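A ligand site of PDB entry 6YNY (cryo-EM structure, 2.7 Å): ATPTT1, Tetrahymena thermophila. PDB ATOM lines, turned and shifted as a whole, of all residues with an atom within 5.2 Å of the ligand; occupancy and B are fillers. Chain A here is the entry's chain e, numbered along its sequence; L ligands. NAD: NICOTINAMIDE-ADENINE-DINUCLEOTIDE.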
ATOM      1  N   VAL A  43     -25.365  32.745  -0.963  1.00  0.00           N
ATOM      2  CA  VAL A  43     -26.757  32.417  -0.636  1.00  0.00           C
ATOM      3  C   VAL A  43     -26.701  31.488   0.564  1.00  0.00           C
ATOM      4  O   VAL A  43     -26.545  30.265   0.430  1.00  0.00           O
ATOM      5  CB  VAL A  43     -27.497  31.780  -1.807  1.00  0.00           C
ATOM      6  CG1 VAL A  43     -28.943  31.526  -1.432  1.00  0.00           C
ATOM      7  CG2 VAL A  43     -27.412  32.673  -3.031  1.00  0.00           C
ATOM      8  N   GLY A  44     -26.829  32.055   1.746  1.00  0.00           N
ATOM      9  CA  GLY A  44     -26.769  31.310   2.991  1.00  0.00           C
ATOM     10  C   GLY A  44     -25.983  32.080   4.035  1.00  0.00           C
ATOM     11  O   GLY A  44     -25.051  32.826   3.729  1.00  0.00           O
ATOM     12  N   ALA A  45     -26.370  31.895   5.292  1.00  0.00           N
ATOM     13  CA  ALA A  45     -25.741  32.582   6.416  1.00  0.00           C
ATOM     14  C   ALA A  45     -25.028  31.646   7.370  1.00  0.00           C
ATOM     15  O   ALA A  45     -24.018  32.049   7.957  1.00  0.00           O
ATOM     16  CB  ALA A  45     -26.784  33.386   7.195  1.00  0.00           C
ATOM     17  N   ASN A  46     -25.516  30.420   7.545  1.00  0.00           N
ATOM     18  CA  ASN A  46     -24.840  29.475   8.422  1.00  0.00           C
ATOM     19  C   ASN A  46     -23.431  29.181   7.915  1.00  0.00           C
ATOM     20  O   ASN A  46     -22.442  29.431   8.611  1.00  0.00           O
ATOM     21  CB  ASN A  46     -25.661  28.190   8.522  1.00  0.00           C
ATOM     22  CG  ASN A  46     -25.028  27.165   9.444  1.00  0.00           C
ATOM     23  OD1 ASN A  46     -24.232  27.510  10.316  1.00  0.00           O
ATOM     24  ND2 ASN A  46     -25.368  25.900   9.247  1.00  0.00           N
ATOM     25  N   LEU A  47     -23.334  28.645   6.702  1.00  0.00           N
ATOM     26  CA  LEU A  47     -22.053  28.402   6.066  1.00  0.00           C
ATOM     27  C   LEU A  47     -21.721  29.434   5.005  1.00  0.00           C
ATOM     28  O   LEU A  47     -20.530  29.678   4.751  1.00  0.00           O
ATOM     29  CB  LEU A  47     -22.029  27.012   5.421  1.00  0.00           C
ATOM     30  CG  LEU A  47     -21.947  25.837   6.396  1.00  0.00           C
ATOM     31  CD1 LEU A  47     -22.137  24.527   5.675  1.00  0.00           C
ATOM     32  CD2 LEU A  47     -20.622  25.845   7.127  1.00  0.00           C
ATOM     33  N   SER A  68     -27.547  36.870   1.034  1.00  0.00           N
ATOM     34  CA  SER A  68     -29.002  36.877   1.116  1.00  0.00           C
ATOM     35  C   SER A  68     -29.459  35.542   1.685  1.00  0.00           C
ATOM     36  O   SER A  68     -29.401  34.519   1.007  1.00  0.00           O
ATOM     37  CB  SER A  68     -29.635  37.110  -0.253  1.00  0.00           C
ATOM     38  OG  SER A  68     -29.283  36.075  -1.144  1.00  0.00           O
ATOM     39  N   PHE A  69     -29.906  35.556   2.939  1.00  0.00           N
ATOM     40  CA  PHE A  69     -30.429  34.373   3.595  1.00  0.00           C
ATOM     41  C   PHE A  69     -31.954  34.450   3.660  1.00  0.00           C
ATOM     42  O   PHE A  69     -32.574  35.413   3.182  1.00  0.00           O
ATOM     43  CB  PHE A  69     -29.824  34.225   4.993  1.00  0.00           C
ATOM     44  CG  PHE A  69     -29.944  35.456   5.843  1.00  0.00           C
ATOM     45  CD1 PHE A  69     -28.905  36.358   5.923  1.00  0.00           C
ATOM     46  CD2 PHE A  69     -31.107  35.707   6.557  1.00  0.00           C
ATOM     47  CE1 PHE A  69     -29.017  37.490   6.698  1.00  0.00           C
ATOM     48  CE2 PHE A  69     -31.218  36.839   7.333  1.00  0.00           C
ATOM     49  CZ  PHE A  69     -30.178  37.735   7.405  1.00  0.00           C
ATOM     50  N   ASP A  70     -32.568  33.435   4.253  1.00  0.00           N
ATOM     51  CA  ASP A  70     -34.017  33.335   4.332  1.00  0.00           C
ATOM     52  C   ASP A  70     -34.528  33.370   5.754  1.00  0.00           C
ATOM     53  O   ASP A  70     -35.528  34.042   6.034  1.00  0.00           O
ATOM     54  CB  ASP A  70     -34.489  32.042   3.640  1.00  0.00           C
ATOM     55  CG  ASP A  70     -35.994  31.961   3.538  1.00  0.00           C
ATOM     56  OD1 ASP A  70     -36.680  32.909   3.960  1.00  0.00           O
ATOM     57  OD2 ASP A  70     -36.498  30.932   3.028  1.00  0.00           O
ATOM     58  N   GLN A  71     -33.875  32.655   6.672  1.00  0.00           N
ATOM     59  CA  GLN A  71     -34.307  32.606   8.058  1.00  0.00           C
ATOM     60  C   GLN A  71     -33.414  33.497   8.917  1.00  0.00           C
ATOM     61  O   GLN A  71     -32.219  33.639   8.643  1.00  0.00           O
ATOM     62  CB  GLN A  71     -34.254  31.165   8.594  1.00  0.00           C
ATOM     63  CG  GLN A  71     -32.862  30.602   8.734  1.00  0.00           C
ATOM     64  CD  GLN A  71     -32.868  29.119   9.021  1.00  0.00           C
ATOM     65  OE1 GLN A  71     -33.929  28.493   9.089  1.00  0.00           O
ATOM     66  NE2 GLN A  71     -31.691  28.544   9.199  1.00  0.00           N
ATOM     67  N   ASN A  74     -30.157  30.790  13.348  1.00  0.00           N
ATOM     68  CA  ASN A  74     -29.410  29.593  12.984  1.00  0.00           C
ATOM     69  C   ASN A  74     -29.174  28.771  14.244  1.00  0.00           C
ATOM     70  O   ASN A  74     -28.314  29.110  15.054  1.00  0.00           O
ATOM     71  CB  ASN A  74     -28.084  29.953  12.319  1.00  0.00           C
ATOM     72  CG  ASN A  74     -28.268  30.866  11.123  1.00  0.00           C
ATOM     73  OD1 ASN A  74     -29.288  30.819  10.439  1.00  0.00           O
ATOM     74  ND2 ASN A  74     -27.268  31.694  10.866  1.00  0.00           N
ATOM     75  N   TYR A  77     -27.167  22.911  15.551  1.00  0.00           N
ATOM     76  CA  TYR A  77     -27.539  21.505  15.633  1.00  0.00           C
ATOM     77  C   TYR A  77     -26.377  20.606  16.008  1.00  0.00           C
ATOM     78  O   TYR A  77     -26.603  19.440  16.349  1.00  0.00           O
ATOM     79  CB  TYR A  77     -28.121  21.053  14.299  1.00  0.00           C
ATOM     80  CG  TYR A  77     -29.324  21.845  13.848  1.00  0.00           C
ATOM     81  CD1 TYR A  77     -30.603  21.452  14.183  1.00  0.00           C
ATOM     82  CD2 TYR A  77     -29.168  22.986  13.084  1.00  0.00           C
ATOM     83  CE1 TYR A  77     -31.698  22.174  13.768  1.00  0.00           C
ATOM     84  CE2 TYR A  77     -30.258  23.722  12.673  1.00  0.00           C
ATOM     85  CZ  TYR A  77     -31.525  23.309  13.013  1.00  0.00           C
ATOM     86  OH  TYR A  77     -32.620  24.031  12.599  1.00  0.00           O
ATOM     87  N   SER A  78     -25.149  21.104  15.956  1.00  0.00           N
ATOM     88  CA  SER A  78     -23.996  20.294  16.348  1.00  0.00           C
ATOM     89  C   SER A  78     -23.960  20.044  17.849  1.00  0.00           C
ATOM     90  O   SER A  78     -23.237  19.153  18.299  1.00  0.00           O
ATOM     91  CB  SER A  78     -22.708  20.967  15.890  1.00  0.00           C
ATOM     92  OG  SER A  78     -22.706  21.146  14.493  1.00  0.00           O
ATOM     93  N   SER A  97     -28.603  35.164  12.191  1.00  0.00           N
ATOM     94  CA  SER A  97     -27.853  35.028  10.945  1.00  0.00           C
ATOM     95  C   SER A  97     -26.923  36.211  10.712  1.00  0.00           C
ATOM     96  O   SER A  97     -25.862  36.056  10.110  1.00  0.00           O
ATOM     97  CB  SER A  97     -28.822  34.875   9.769  1.00  0.00           C
ATOM     98  OG  SER A  97     -29.621  33.715   9.928  1.00  0.00           O
ATOM     99  N   LEU A 110     -34.059  38.101   2.356  1.00  0.00           N
ATOM    100  CA  LEU A 110     -34.988  37.811   1.273  1.00  0.00           C
ATOM    101  C   LEU A 110     -34.454  36.652   0.463  1.00  0.00           C
ATOM    102  O   LEU A 110     -33.311  36.686  -0.006  1.00  0.00           O
ATOM    103  CB  LEU A 110     -35.197  39.037   0.379  1.00  0.00           C
ATOM    104  CG  LEU A 110     -35.943  40.220   1.015  1.00  0.00           C
ATOM    105  CD1 LEU A 110     -36.074  41.356   0.012  1.00  0.00           C
ATOM    106  CD2 LEU A 110     -37.311  39.798   1.502  1.00  0.00           C
ATOM    107  N   ALA A 111     -35.287  35.624   0.299  1.00  0.00           N
ATOM    108  CA  ALA A 111     -34.873  34.433  -0.441  1.00  0.00           C
ATOM    109  C   ALA A 111     -34.913  34.700  -1.943  1.00  0.00           C
ATOM    110  O   ALA A 111     -35.679  35.522  -2.434  1.00  0.00           O
ATOM    111  CB  ALA A 111     -35.775  33.248  -0.097  1.00  0.00           C
ATOM    112  N   VAL A 112     -34.056  33.970  -2.671  1.00  0.00           N
ATOM    113  CA  VAL A 112     -33.988  34.139  -4.114  1.00  0.00           C
ATOM    114  C   VAL A 112     -35.204  33.484  -4.753  1.00  0.00           C
ATOM    115  O   VAL A 112     -35.514  32.312  -4.512  1.00  0.00           O
ATOM    116  CB  VAL A 112     -32.687  33.531  -4.656  1.00  0.00           C
ATOM    117  CG1 VAL A 112     -31.488  34.128  -3.933  1.00  0.00           C
ATOM    118  CG2 VAL A 112     -32.691  32.019  -4.515  1.00  0.00           C
ATOM    119  N   ALA A 138     -25.324  27.975  -0.549  1.00  0.00           N
ATOM    120  CA  ALA A 138     -25.291  27.256   0.723  1.00  0.00           C
ATOM    121  C   ALA A 138     -26.693  27.143   1.290  1.00  0.00           C
ATOM    122  O   ALA A 138     -26.903  27.223   2.505  1.00  0.00           O
ATOM    123  CB  ALA A 138     -24.359  27.934   1.710  1.00  0.00           C
ATOM    124  N   THR A 139     -27.681  26.968   0.415  1.00  0.00           N
ATOM    125  CA  THR A 139     -29.070  26.865   0.846  1.00  0.00           C
ATOM    126  C   THR A 139     -29.335  25.622   1.674  1.00  0.00           C
ATOM    127  O   THR A 139     -30.371  25.556   2.356  1.00  0.00           O
ATOM    128  CB  THR A 139     -29.999  26.888  -0.363  1.00  0.00           C
ATOM    129  OG1 THR A 139     -29.633  25.827  -1.257  1.00  0.00           O
ATOM    130  CG2 THR A 139     -29.898  28.217  -1.081  1.00  0.00           C
ATOM    131  N   GLY A 140     -28.440  24.641   1.639  1.00  0.00           N
ATOM    132  CA  GLY A 140     -28.608  23.438   2.425  1.00  0.00           C
ATOM    133  C   GLY A 140     -29.964  22.776   2.224  1.00  0.00           C
ATOM    134  O   GLY A 140     -30.623  22.995   1.201  1.00  0.00           O
ATOM    135  N   LEU A 141     -30.386  21.983   3.204  1.00  0.00           N
ATOM    136  CA  LEU A 141     -31.656  21.266   3.141  1.00  0.00           C
ATOM    137  C   LEU A 141     -32.693  22.026   3.943  1.00  0.00           C
ATOM    138  O   LEU A 141     -32.522  22.243   5.150  1.00  0.00           O
ATOM    139  CB  LEU A 141     -31.489  19.837   3.673  1.00  0.00           C
ATOM    140  CG  LEU A 141     -30.470  18.987   2.928  1.00  0.00           C
ATOM    141  CD1 LEU A 141     -30.270  17.654   3.635  1.00  0.00           C
ATOM    142  CD2 LEU A 141     -30.912  18.763   1.497  1.00  0.00           C
ATOM    143  N   LYS A 142     -33.761  22.440   3.276  1.00  0.00           N
ATOM    144  CA  LYS A 142     -34.804  23.227   3.925  1.00  0.00           C
ATOM    145  C   LYS A 142     -35.788  22.304   4.641  1.00  0.00           C
ATOM    146  O   LYS A 142     -36.328  21.366   4.038  1.00  0.00           O
ATOM    147  CB  LYS A 142     -35.536  24.080   2.893  1.00  0.00           C
ATOM    148  CG  LYS A 142     -36.214  25.301   3.472  1.00  0.00           C
ATOM    149  CD  LYS A 142     -36.962  26.074   2.411  1.00  0.00           C
ATOM    150  CE  LYS A 142     -37.452  27.408   2.943  1.00  0.00           C
ATOM    151  NZ  LYS A 142     -38.281  28.134   1.932  1.00  0.00           N
ATOM    152  N   HIS A 143     -36.024  22.574   5.917  1.00  0.00           N
ATOM    153  CA  HIS A 143     -36.969  21.791   6.694  1.00  0.00           C
ATOM    154  C   HIS A 143     -38.389  22.075   6.243  1.00  0.00           C
ATOM    155  O   HIS A 143     -38.756  23.235   6.013  1.00  0.00           O
ATOM    156  CB  HIS A 143     -36.809  22.094   8.181  1.00  0.00           C
ATOM    157  CG  HIS A 143     -35.576  21.516   8.789  1.00  0.00           C
ATOM    158  ND1 HIS A 143     -35.093  21.914  10.019  1.00  0.00           N
ATOM    159  CD2 HIS A 143     -34.733  20.554   8.352  1.00  0.00           C
ATOM    160  CE1 HIS A 143     -34.001  21.235  10.307  1.00  0.00           C
ATOM    161  NE2 HIS A 143     -33.757  20.397   9.314  1.00  0.00           N
ATOM    162  N   ASN A 165     -36.365  17.650  16.166  1.00  0.00           N
ATOM    163  CA  ASN A 165     -34.923  17.875  16.179  1.00  0.00           C
ATOM    164  C   ASN A 165     -34.551  19.330  16.396  1.00  0.00           C
ATOM    165  O   ASN A 165     -33.409  19.612  16.766  1.00  0.00           O
ATOM    166  CB  ASN A 165     -34.309  17.387  14.873  1.00  0.00           C
ATOM    167  CG  ASN A 165     -32.810  17.371  14.910  1.00  0.00           C
ATOM    168  OD1 ASN A 165     -32.207  17.399  15.982  1.00  0.00           O
ATOM    169  ND2 ASN A 165     -32.191  17.303  13.743  1.00  0.00           N
ATOM    170  N   ALA A 200     -31.204  16.402   7.039  1.00  0.00           N
ATOM    171  CA  ALA A 200     -30.195  17.092   7.835  1.00  0.00           C
ATOM    172  C   ALA A 200     -30.115  16.491   9.227  1.00  0.00           C
ATOM    173  O   ALA A 200     -31.128  16.156   9.834  1.00  0.00           O
ATOM    174  CB  ALA A 200     -30.520  18.583   7.928  1.00  0.00           C
ATOM    175  N   GLY A 201     -28.890  16.338   9.720  1.00  0.00           N
ATOM    176  CA  GLY A 201     -28.677  15.809  11.049  1.00  0.00           C
ATOM    177  C   GLY A 201     -28.577  14.295  11.053  1.00  0.00           C
ATOM    178  O   GLY A 201     -29.274  13.620  11.824  1.00  0.00           O
ATOM    179  N   GLU A 204     -25.440  13.819  13.992  1.00  0.00           N
ATOM    180  CA  GLU A 204     -25.424  14.794  15.074  1.00  0.00           C
ATOM    181  C   GLU A 204     -26.754  14.905  15.796  1.00  0.00           C
ATOM    182  O   GLU A 204     -26.854  15.666  16.772  1.00  0.00           O
ATOM    183  CB  GLU A 204     -25.012  16.166  14.531  1.00  0.00           C
ATOM    184  CG  GLU A 204     -25.961  16.732  13.488  1.00  0.00           C
ATOM    185  CD  GLU A 204     -25.470  18.050  12.911  1.00  0.00           C
ATOM    186  OE1 GLU A 204     -24.379  18.501  13.304  1.00  0.00           O
ATOM    187  OE2 GLU A 204     -26.188  18.634  12.062  1.00  0.00           O
ATOM    188  N   CYS A 205     -27.778  14.191  15.342  1.00  0.00           N
ATOM    189  CA  CYS A 205     -29.099  14.248  15.954  1.00  0.00           C
ATOM    190  C   CYS A 205     -29.600  12.858  16.353  1.00  0.00           C
ATOM    191  O   CYS A 205     -30.804  12.687  16.597  1.00  0.00           O
ATOM    192  CB  CYS A 205     -30.101  14.921  15.009  1.00  0.00           C
ATOM    193  SG  CYS A 205     -29.618  16.588  14.537  1.00  0.00           S
ATOM    194  N   ILE A 298     -36.755  13.360  13.260  1.00  0.00           N
ATOM    195  CA  ILE A 298     -35.865  14.319  12.616  1.00  0.00           C
ATOM    196  C   ILE A 298     -36.634  15.024  11.517  1.00  0.00           C
ATOM    197  O   ILE A 298     -37.213  14.383  10.638  1.00  0.00           O
ATOM    198  CB  ILE A 298     -34.614  13.620  12.075  1.00  0.00           C
ATOM    199  CG1 ILE A 298     -33.826  12.990  13.221  1.00  0.00           C
ATOM    200  CG2 ILE A 298     -33.750  14.604  11.315  1.00  0.00           C
ATOM    201  CD1 ILE A 298     -32.638  12.188  12.792  1.00  0.00           C
ATOM    202  N   GLN A 304     -35.989  22.444  -3.172  1.00  0.00           N
ATOM    203  CA  GLN A 304     -36.535  23.721  -3.593  1.00  0.00           C
ATOM    204  C   GLN A 304     -36.596  23.758  -5.120  1.00  0.00           C
ATOM    205  O   GLN A 304     -35.639  23.377  -5.790  1.00  0.00           O
ATOM    206  CB  GLN A 304     -35.687  24.867  -3.055  1.00  0.00           C
ATOM    207  CG  GLN A 304     -35.392  24.746  -1.562  1.00  0.00           C
ATOM    208  CD  GLN A 304     -34.691  25.952  -0.994  1.00  0.00           C
ATOM    209  OE1 GLN A 304     -35.266  27.035  -0.897  1.00  0.00           O
ATOM    210  NE2 GLN A 304     -33.435  25.781  -0.598  1.00  0.00           N
ATOM    211  N   PHE A 306     -36.848  26.291  -7.313  1.00  0.00           N
ATOM    212  CA  PHE A 306     -36.057  27.276  -8.047  1.00  0.00           C
ATOM    213  C   PHE A 306     -34.681  26.745  -8.417  1.00  0.00           C
ATOM    214  O   PHE A 306     -34.058  27.285  -9.338  1.00  0.00           O
ATOM    215  CB  PHE A 306     -35.923  28.567  -7.229  1.00  0.00           C
ATOM    216  CG  PHE A 306     -34.974  28.460  -6.078  1.00  0.00           C
ATOM    217  CD1 PHE A 306     -35.405  27.965  -4.862  1.00  0.00           C
ATOM    218  CD2 PHE A 306     -33.664  28.854  -6.213  1.00  0.00           C
ATOM    219  CE1 PHE A 306     -34.528  27.868  -3.797  1.00  0.00           C
ATOM    220  CE2 PHE A 306     -32.781  28.764  -5.153  1.00  0.00           C
ATOM    221  CZ  PHE A 306     -33.220  28.266  -3.949  1.00  0.00           C
ATOM    222  N   LEU A 337     -21.799  24.279  -1.701  1.00  0.00           N
ATOM    223  CA  LEU A 337     -21.243  23.582  -0.552  1.00  0.00           C
ATOM    224  C   LEU A 337     -22.321  23.404   0.502  1.00  0.00           C
ATOM    225  O   LEU A 337     -23.478  23.816   0.317  1.00  0.00           O
ATOM    226  CB  LEU A 337     -20.050  24.345   0.033  1.00  0.00           C
ATOM    227  CG  LEU A 337     -20.380  25.569   0.891  1.00  0.00           C
ATOM    228  CD1 LEU A 337     -19.113  26.272   1.304  1.00  0.00           C
ATOM    229  CD2 LEU A 337     -21.312  26.512   0.167  1.00  0.00           C
ATOM    230  N   GLY A 338     -21.953  22.772   1.603  1.00  0.00           N
ATOM    231  CA  GLY A 338     -22.876  22.568   2.706  1.00  0.00           C
ATOM    232  C   GLY A 338     -23.655  21.277   2.531  1.00  0.00           C
ATOM    233  O   GLY A 338     -23.086  20.235   2.218  1.00  0.00           O
ATOM    234  N   ASP A 339     -24.968  21.351   2.740  1.00  0.00           N
ATOM    235  CA  ASP A 339     -25.825  20.193   2.613  1.00  0.00           C
ATOM    236  C   ASP A 339     -26.468  20.076   1.243  1.00  0.00           C
ATOM    237  O   ASP A 339     -26.743  18.963   0.776  1.00  0.00           O
ATOM    238  CB  ASP A 339     -26.925  20.238   3.677  1.00  0.00           C
ATOM    239  CG  ASP A 339     -26.374  20.322   5.085  1.00  0.00           C
ATOM    240  OD1 ASP A 339     -25.134  20.337   5.235  1.00  0.00           O
ATOM    241  OD2 ASP A 339     -27.170  20.392   6.037  1.00  0.00           O
ATOM    242  N   ALA A 340     -26.717  21.213   0.570  1.00  0.00           N
ATOM    243  CA  ALA A 340     -27.329  21.180  -0.747  1.00  0.00           C
ATOM    244  C   ALA A 340     -26.425  20.550  -1.796  1.00  0.00           C
ATOM    245  O   ALA A 340     -26.908  20.153  -2.858  1.00  0.00           O
ATOM    246  CB  ALA A 340     -27.707  22.596  -1.176  1.00  0.00           C
ATOM    247  N   LYS A 347     -23.020  14.806   5.600  1.00  0.00           N
ATOM    248  CA  LYS A 347     -23.295  16.238   5.619  1.00  0.00           C
ATOM    249  C   LYS A 347     -23.218  16.737   7.050  1.00  0.00           C
ATOM    250  O   LYS A 347     -24.224  16.891   7.753  1.00  0.00           O
ATOM    251  CB  LYS A 347     -24.648  16.519   4.987  1.00  0.00           C
ATOM    252  CG  LYS A 347     -24.831  15.879   3.628  1.00  0.00           C
ATOM    253  CD  LYS A 347     -26.116  16.313   2.960  1.00  0.00           C
ATOM    254  CE  LYS A 347     -26.353  15.533   1.693  1.00  0.00           C
ATOM    255  NZ  LYS A 347     -25.223  15.667   0.736  1.00  0.00           N
ATOM    256  N   THR A 348     -22.001  16.997   7.490  1.00  0.00           N
ATOM    257  CA  THR A 348     -21.706  17.487   8.835  1.00  0.00           C
ATOM    258  C   THR A 348     -21.268  18.947   8.759  1.00  0.00           C
ATOM    259  O   THR A 348     -21.281  19.570   7.700  1.00  0.00           O
ATOM    260  CB  THR A 348     -20.618  16.633   9.486  1.00  0.00           C
ATOM    261  OG1 THR A 348     -19.393  16.783   8.780  1.00  0.00           O
ATOM    262  CG2 THR A 348     -21.032  15.180   9.495  1.00  0.00           C
ATOM    263  N   PHE A 349     -20.893  19.491   9.917  1.00  0.00           N
ATOM    264  CA  PHE A 349     -20.419  20.864   9.983  1.00  0.00           C
ATOM    265  C   PHE A 349     -18.911  20.939   9.766  1.00  0.00           C
ATOM    266  O   PHE A 349     -18.436  21.789   9.009  1.00  0.00           O
ATOM    267  CB  PHE A 349     -20.787  21.482  11.330  1.00  0.00           C
ATOM    268  CG  PHE A 349     -20.554  22.965  11.396  1.00  0.00           C
ATOM    269  CD1 PHE A 349     -21.516  23.845  10.940  1.00  0.00           C
ATOM    270  CD2 PHE A 349     -19.383  23.465  11.906  1.00  0.00           C
ATOM    271  CE1 PHE A 349     -21.307  25.195  10.994  1.00  0.00           C
ATOM    272  CE2 PHE A 349     -19.161  24.824  11.967  1.00  0.00           C
ATOM    273  CZ  PHE A 349     -20.127  25.691  11.508  1.00  0.00           C
HETATM  274  PA  NAD L   1     -28.663  25.651   6.535  1.00  0.00           P
HETATM  275  O1A NAD L   1     -27.734  26.390   7.460  1.00  0.00           O
HETATM  276  O2A NAD L   1     -29.571  24.761   7.341  1.00  0.00           O
HETATM  277  O5B NAD L   1     -29.575  26.743   5.654  1.00  0.00           O
HETATM  278  C5B NAD L   1     -28.868  27.505   4.671  1.00  0.00           C
HETATM  279  C4B NAD L   1     -28.968  29.055   4.885  1.00  0.00           C
HETATM  280  O4B NAD L   1     -29.513  29.701   3.507  1.00  0.00           O
HETATM  281  C3B NAD L   1     -29.836  29.389   5.792  1.00  0.00           C
HETATM  282  O3B NAD L   1     -29.537  30.775   6.287  1.00  0.00           O
HETATM  283  C2B NAD L   1     -31.171  29.380   5.008  1.00  0.00           C
HETATM  284  O2B NAD L   1     -32.108  30.147   5.640  1.00  0.00           O
HETATM  285  C1B NAD L   1     -30.787  30.010   3.686  1.00  0.00           C
HETATM  286  N9A NAD L   1     -31.603  29.457   2.616  1.00  0.00           N
HETATM  287  C8A NAD L   1     -32.138  28.296   2.274  1.00  0.00           C
HETATM  288  N7A NAD L   1     -32.815  28.481   1.119  1.00  0.00           N
HETATM  289  C5A NAD L   1     -32.684  29.783   0.769  1.00  0.00           C
HETATM  290  C6A NAD L   1     -33.179  30.508  -0.314  1.00  0.00           C
HETATM  291  N6A NAD L   1     -34.020  30.120  -1.484  1.00  0.00           N
HETATM  292  N1A NAD L   1     -32.909  31.794  -0.433  1.00  0.00           N
HETATM  293  C2A NAD L   1     -32.133  32.422   0.517  1.00  0.00           C
HETATM  294  N3A NAD L   1     -31.656  31.731   1.569  1.00  0.00           N
HETATM  295  C4A NAD L   1     -31.936  30.401   1.695  1.00  0.00           C
HETATM  296  O3  NAD L   1     -27.786  24.761   5.473  1.00  0.00           O
HETATM  297  PN  NAD L   1     -26.145  24.403   5.684  1.00  0.00           P
HETATM  298  O1N NAD L   1     -25.772  23.205   4.786  1.00  0.00           O
HETATM  299  O2N NAD L   1     -25.311  25.588   5.289  1.00  0.00           O
HETATM  300  O5D NAD L   1     -25.844  24.018   7.237  1.00  0.00           O
HETATM  301  C5D NAD L   1     -24.566  23.496   7.520  1.00  0.00           C
HETATM  302  C4D NAD L   1     -24.640  22.587   8.732  1.00  0.00           C
HETATM  303  O4D NAD L   1     -25.919  22.977   9.626  1.00  0.00           O
HETATM  304  C3D NAD L   1     -24.839  21.340   8.362  1.00  0.00           C
HETATM  305  O3D NAD L   1     -23.495  20.648   8.117  1.00  0.00           O
HETATM  306  C2D NAD L   1     -25.534  20.729   9.537  1.00  0.00           C
HETATM  307  O2D NAD L   1     -24.617  20.139  10.386  1.00  0.00           O
HETATM  308  C1D NAD L   1     -26.244  21.929  10.257  1.00  0.00           C
HETATM  309  N1N NAD L   1     -27.729  21.749  10.200  1.00  0.00           N
HETATM  310  C2N NAD L   1     -28.324  20.704  10.874  1.00  0.00           C
HETATM  311  C3N NAD L   1     -29.702  20.535  10.827  1.00  0.00           C
HETATM  312  C7N NAD L   1     -30.345  19.330  11.610  1.00  0.00           C
HETATM  313  O7N NAD L   1     -31.513  19.113  11.533  1.00  0.00           O
HETATM  314  N7N NAD L   1     -29.460  18.473  12.450  1.00  0.00           N
HETATM  315  C4N NAD L   1     -30.480  21.394  10.107  1.00  0.00           C
HETATM  316  C5N NAD L   1     -29.893  22.443   9.429  1.00  0.00           C
HETATM  317  C6N NAD L   1     -28.503  22.622   9.483  1.00  0.00           C
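An oxygen (O3D) of the ligand sits at hydrogen-bond distance from the backbone carbonyl oxygen (O) of Thr 348 (2.5 Å). An oxygen (O2D) of the ligand is in hydrogen-bond range of the side-chain carboxylate (OE2) of Glu 204, at 2.7 Å. The side-chain amide nitrogen (ND2) of Asn 46 is in hydrogen-bond range of an oxygen (O5D) of the ligand, 2.8 Å away. N7N of the ligand lies within hydrogen-bond range of SG of Cys 205 (2.8 Å). The backbone NH (N) of Asp 339 lies within hydrogen-bond range of an oxygen (O1N) of the ligand (2.9 Å). The side-chain carboxylate of Asp 339 sits close to an oxygen (O3D) of the ligand, 3.3 Å away. The side-chain amide nitrogen (ND2) of Asn 165 sits at hydrogen-bond distance from an oxygen (O7N) of the ligand, at 2.9 Å. The backbone NH (N) of Gln 71 lies close to an oxygen (O2B) of the ligand, 3.2 Å away. The side-chain amide nitrogen of Gln 304 sits at hydrogen-bond distance from a nitrogen (N7A) of the ligand, at 3.3 Å. N of Asp 70 sits at hydrogen-bond distance from N3A of the ligand (3.3 Å). The backbone NH (N) of Val 112 lies within hydrogen-bond range of a nitrogen (N1A) of the ligand (3.3 Å). The backbone NH (N) of Phe 349 is in hydrogen-bond range of an oxygen (O3D) of the ligand. A ring nitrogen (NE2) of His 143 sits at hydrogen-bond distance from an oxygen (O7N) of the ligand, 3.4 Å away.
The side-chain carboxylate (OE1) of Glu 204 sits at hydrogen-bond distance from the side-chain hydroxyl (OG) of Ser 78 (3.3 Å). The side-chain amide nitrogen of Asn 165 lies within hydrogen-bond range of the side-chain sulfur of Cys 205 (2.8 Å). The backbone NH (N) of Ala 138 sits at hydrogen-bond distance from the backbone carbonyl oxygen (O) of Val 43 (2.8 Å). The backbone carbonyl oxygen (O) of Gln 71 sits at hydrogen-bond distance from the side-chain hydroxyl (OG) of Ser 97. The backbone NH of Thr 139 lies within hydrogen-bond range of the backbone carbonyl oxygen of Val 43, 3.5 Å away. The side-chain amino group (NZ) of Lys 142 lies within salt-bridge range of the side-chain carboxylate (OD2) of Asp 70 (3.5 Å). N of Leu 110 sits at hydrogen-bond distance from O of Phe 69, 3.2 Å away.
The backbone carbonyl oxygen of Ala 200 lies close to an oxygen (O7N) of the ligand, at 3.4 Å. Val 43 touches the ligand (CG1 to C2A, 3.8 Å). Gly 44 touches the ligand (CA to O4B, 3.2 Å). N of Ala 45 touches O3B of the ligand (3.5 Å). CD1 of Leu 47 touches C5D of the ligand, 3.2 Å away. Ser 68 touches the ligand (O to C2A, 3.5 Å). Phe 69 touches the ligand. CD2 of Tyr 77 touches C2N of the ligand, 3.3 Å away. CB of Ala 111 touches N1A of the ligand, at 3.2 Å. Ala 138 touches the ligand. Thr 139 touches the ligand (O to C8A, 3.3 Å). CA of Gly 140 touches O3 of the ligand, 3.4 Å away. Gly 201 touches the ligand. CZ of Phe 306 touches N6A of the ligand (3.2 Å). CA of Gly 338 touches O1N of the ligand (3.6 Å). O of Lys 347 touches O3D of the ligand (3.8 Å). Hydrophobic or aromatic side chains that line the ligand: Val 43, Ala 45, Leu 47, Phe 69, Tyr 77, Ala 111, Val 112, His 143, Ala 200 and Phe 306. Within 4 Å of the ligand: Val 43, Gly 44, Ala 45, Asn 46, Leu 47, Ser 68, Phe 69, Asp 70, Gln 71, Tyr 77, Ala 111, Val 112, Ala 138, Thr 139, Gly 140, His 143, Asn 165, Ala 200, Gly 201, Glu 204, Cys 205, Gln 304, Phe 306, Gly 338, Asp 339, Lys 347, Thr 348 and Phe 349. The nearest printed residue that does not touch the ligand is Asn 74 (4.2 Å).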
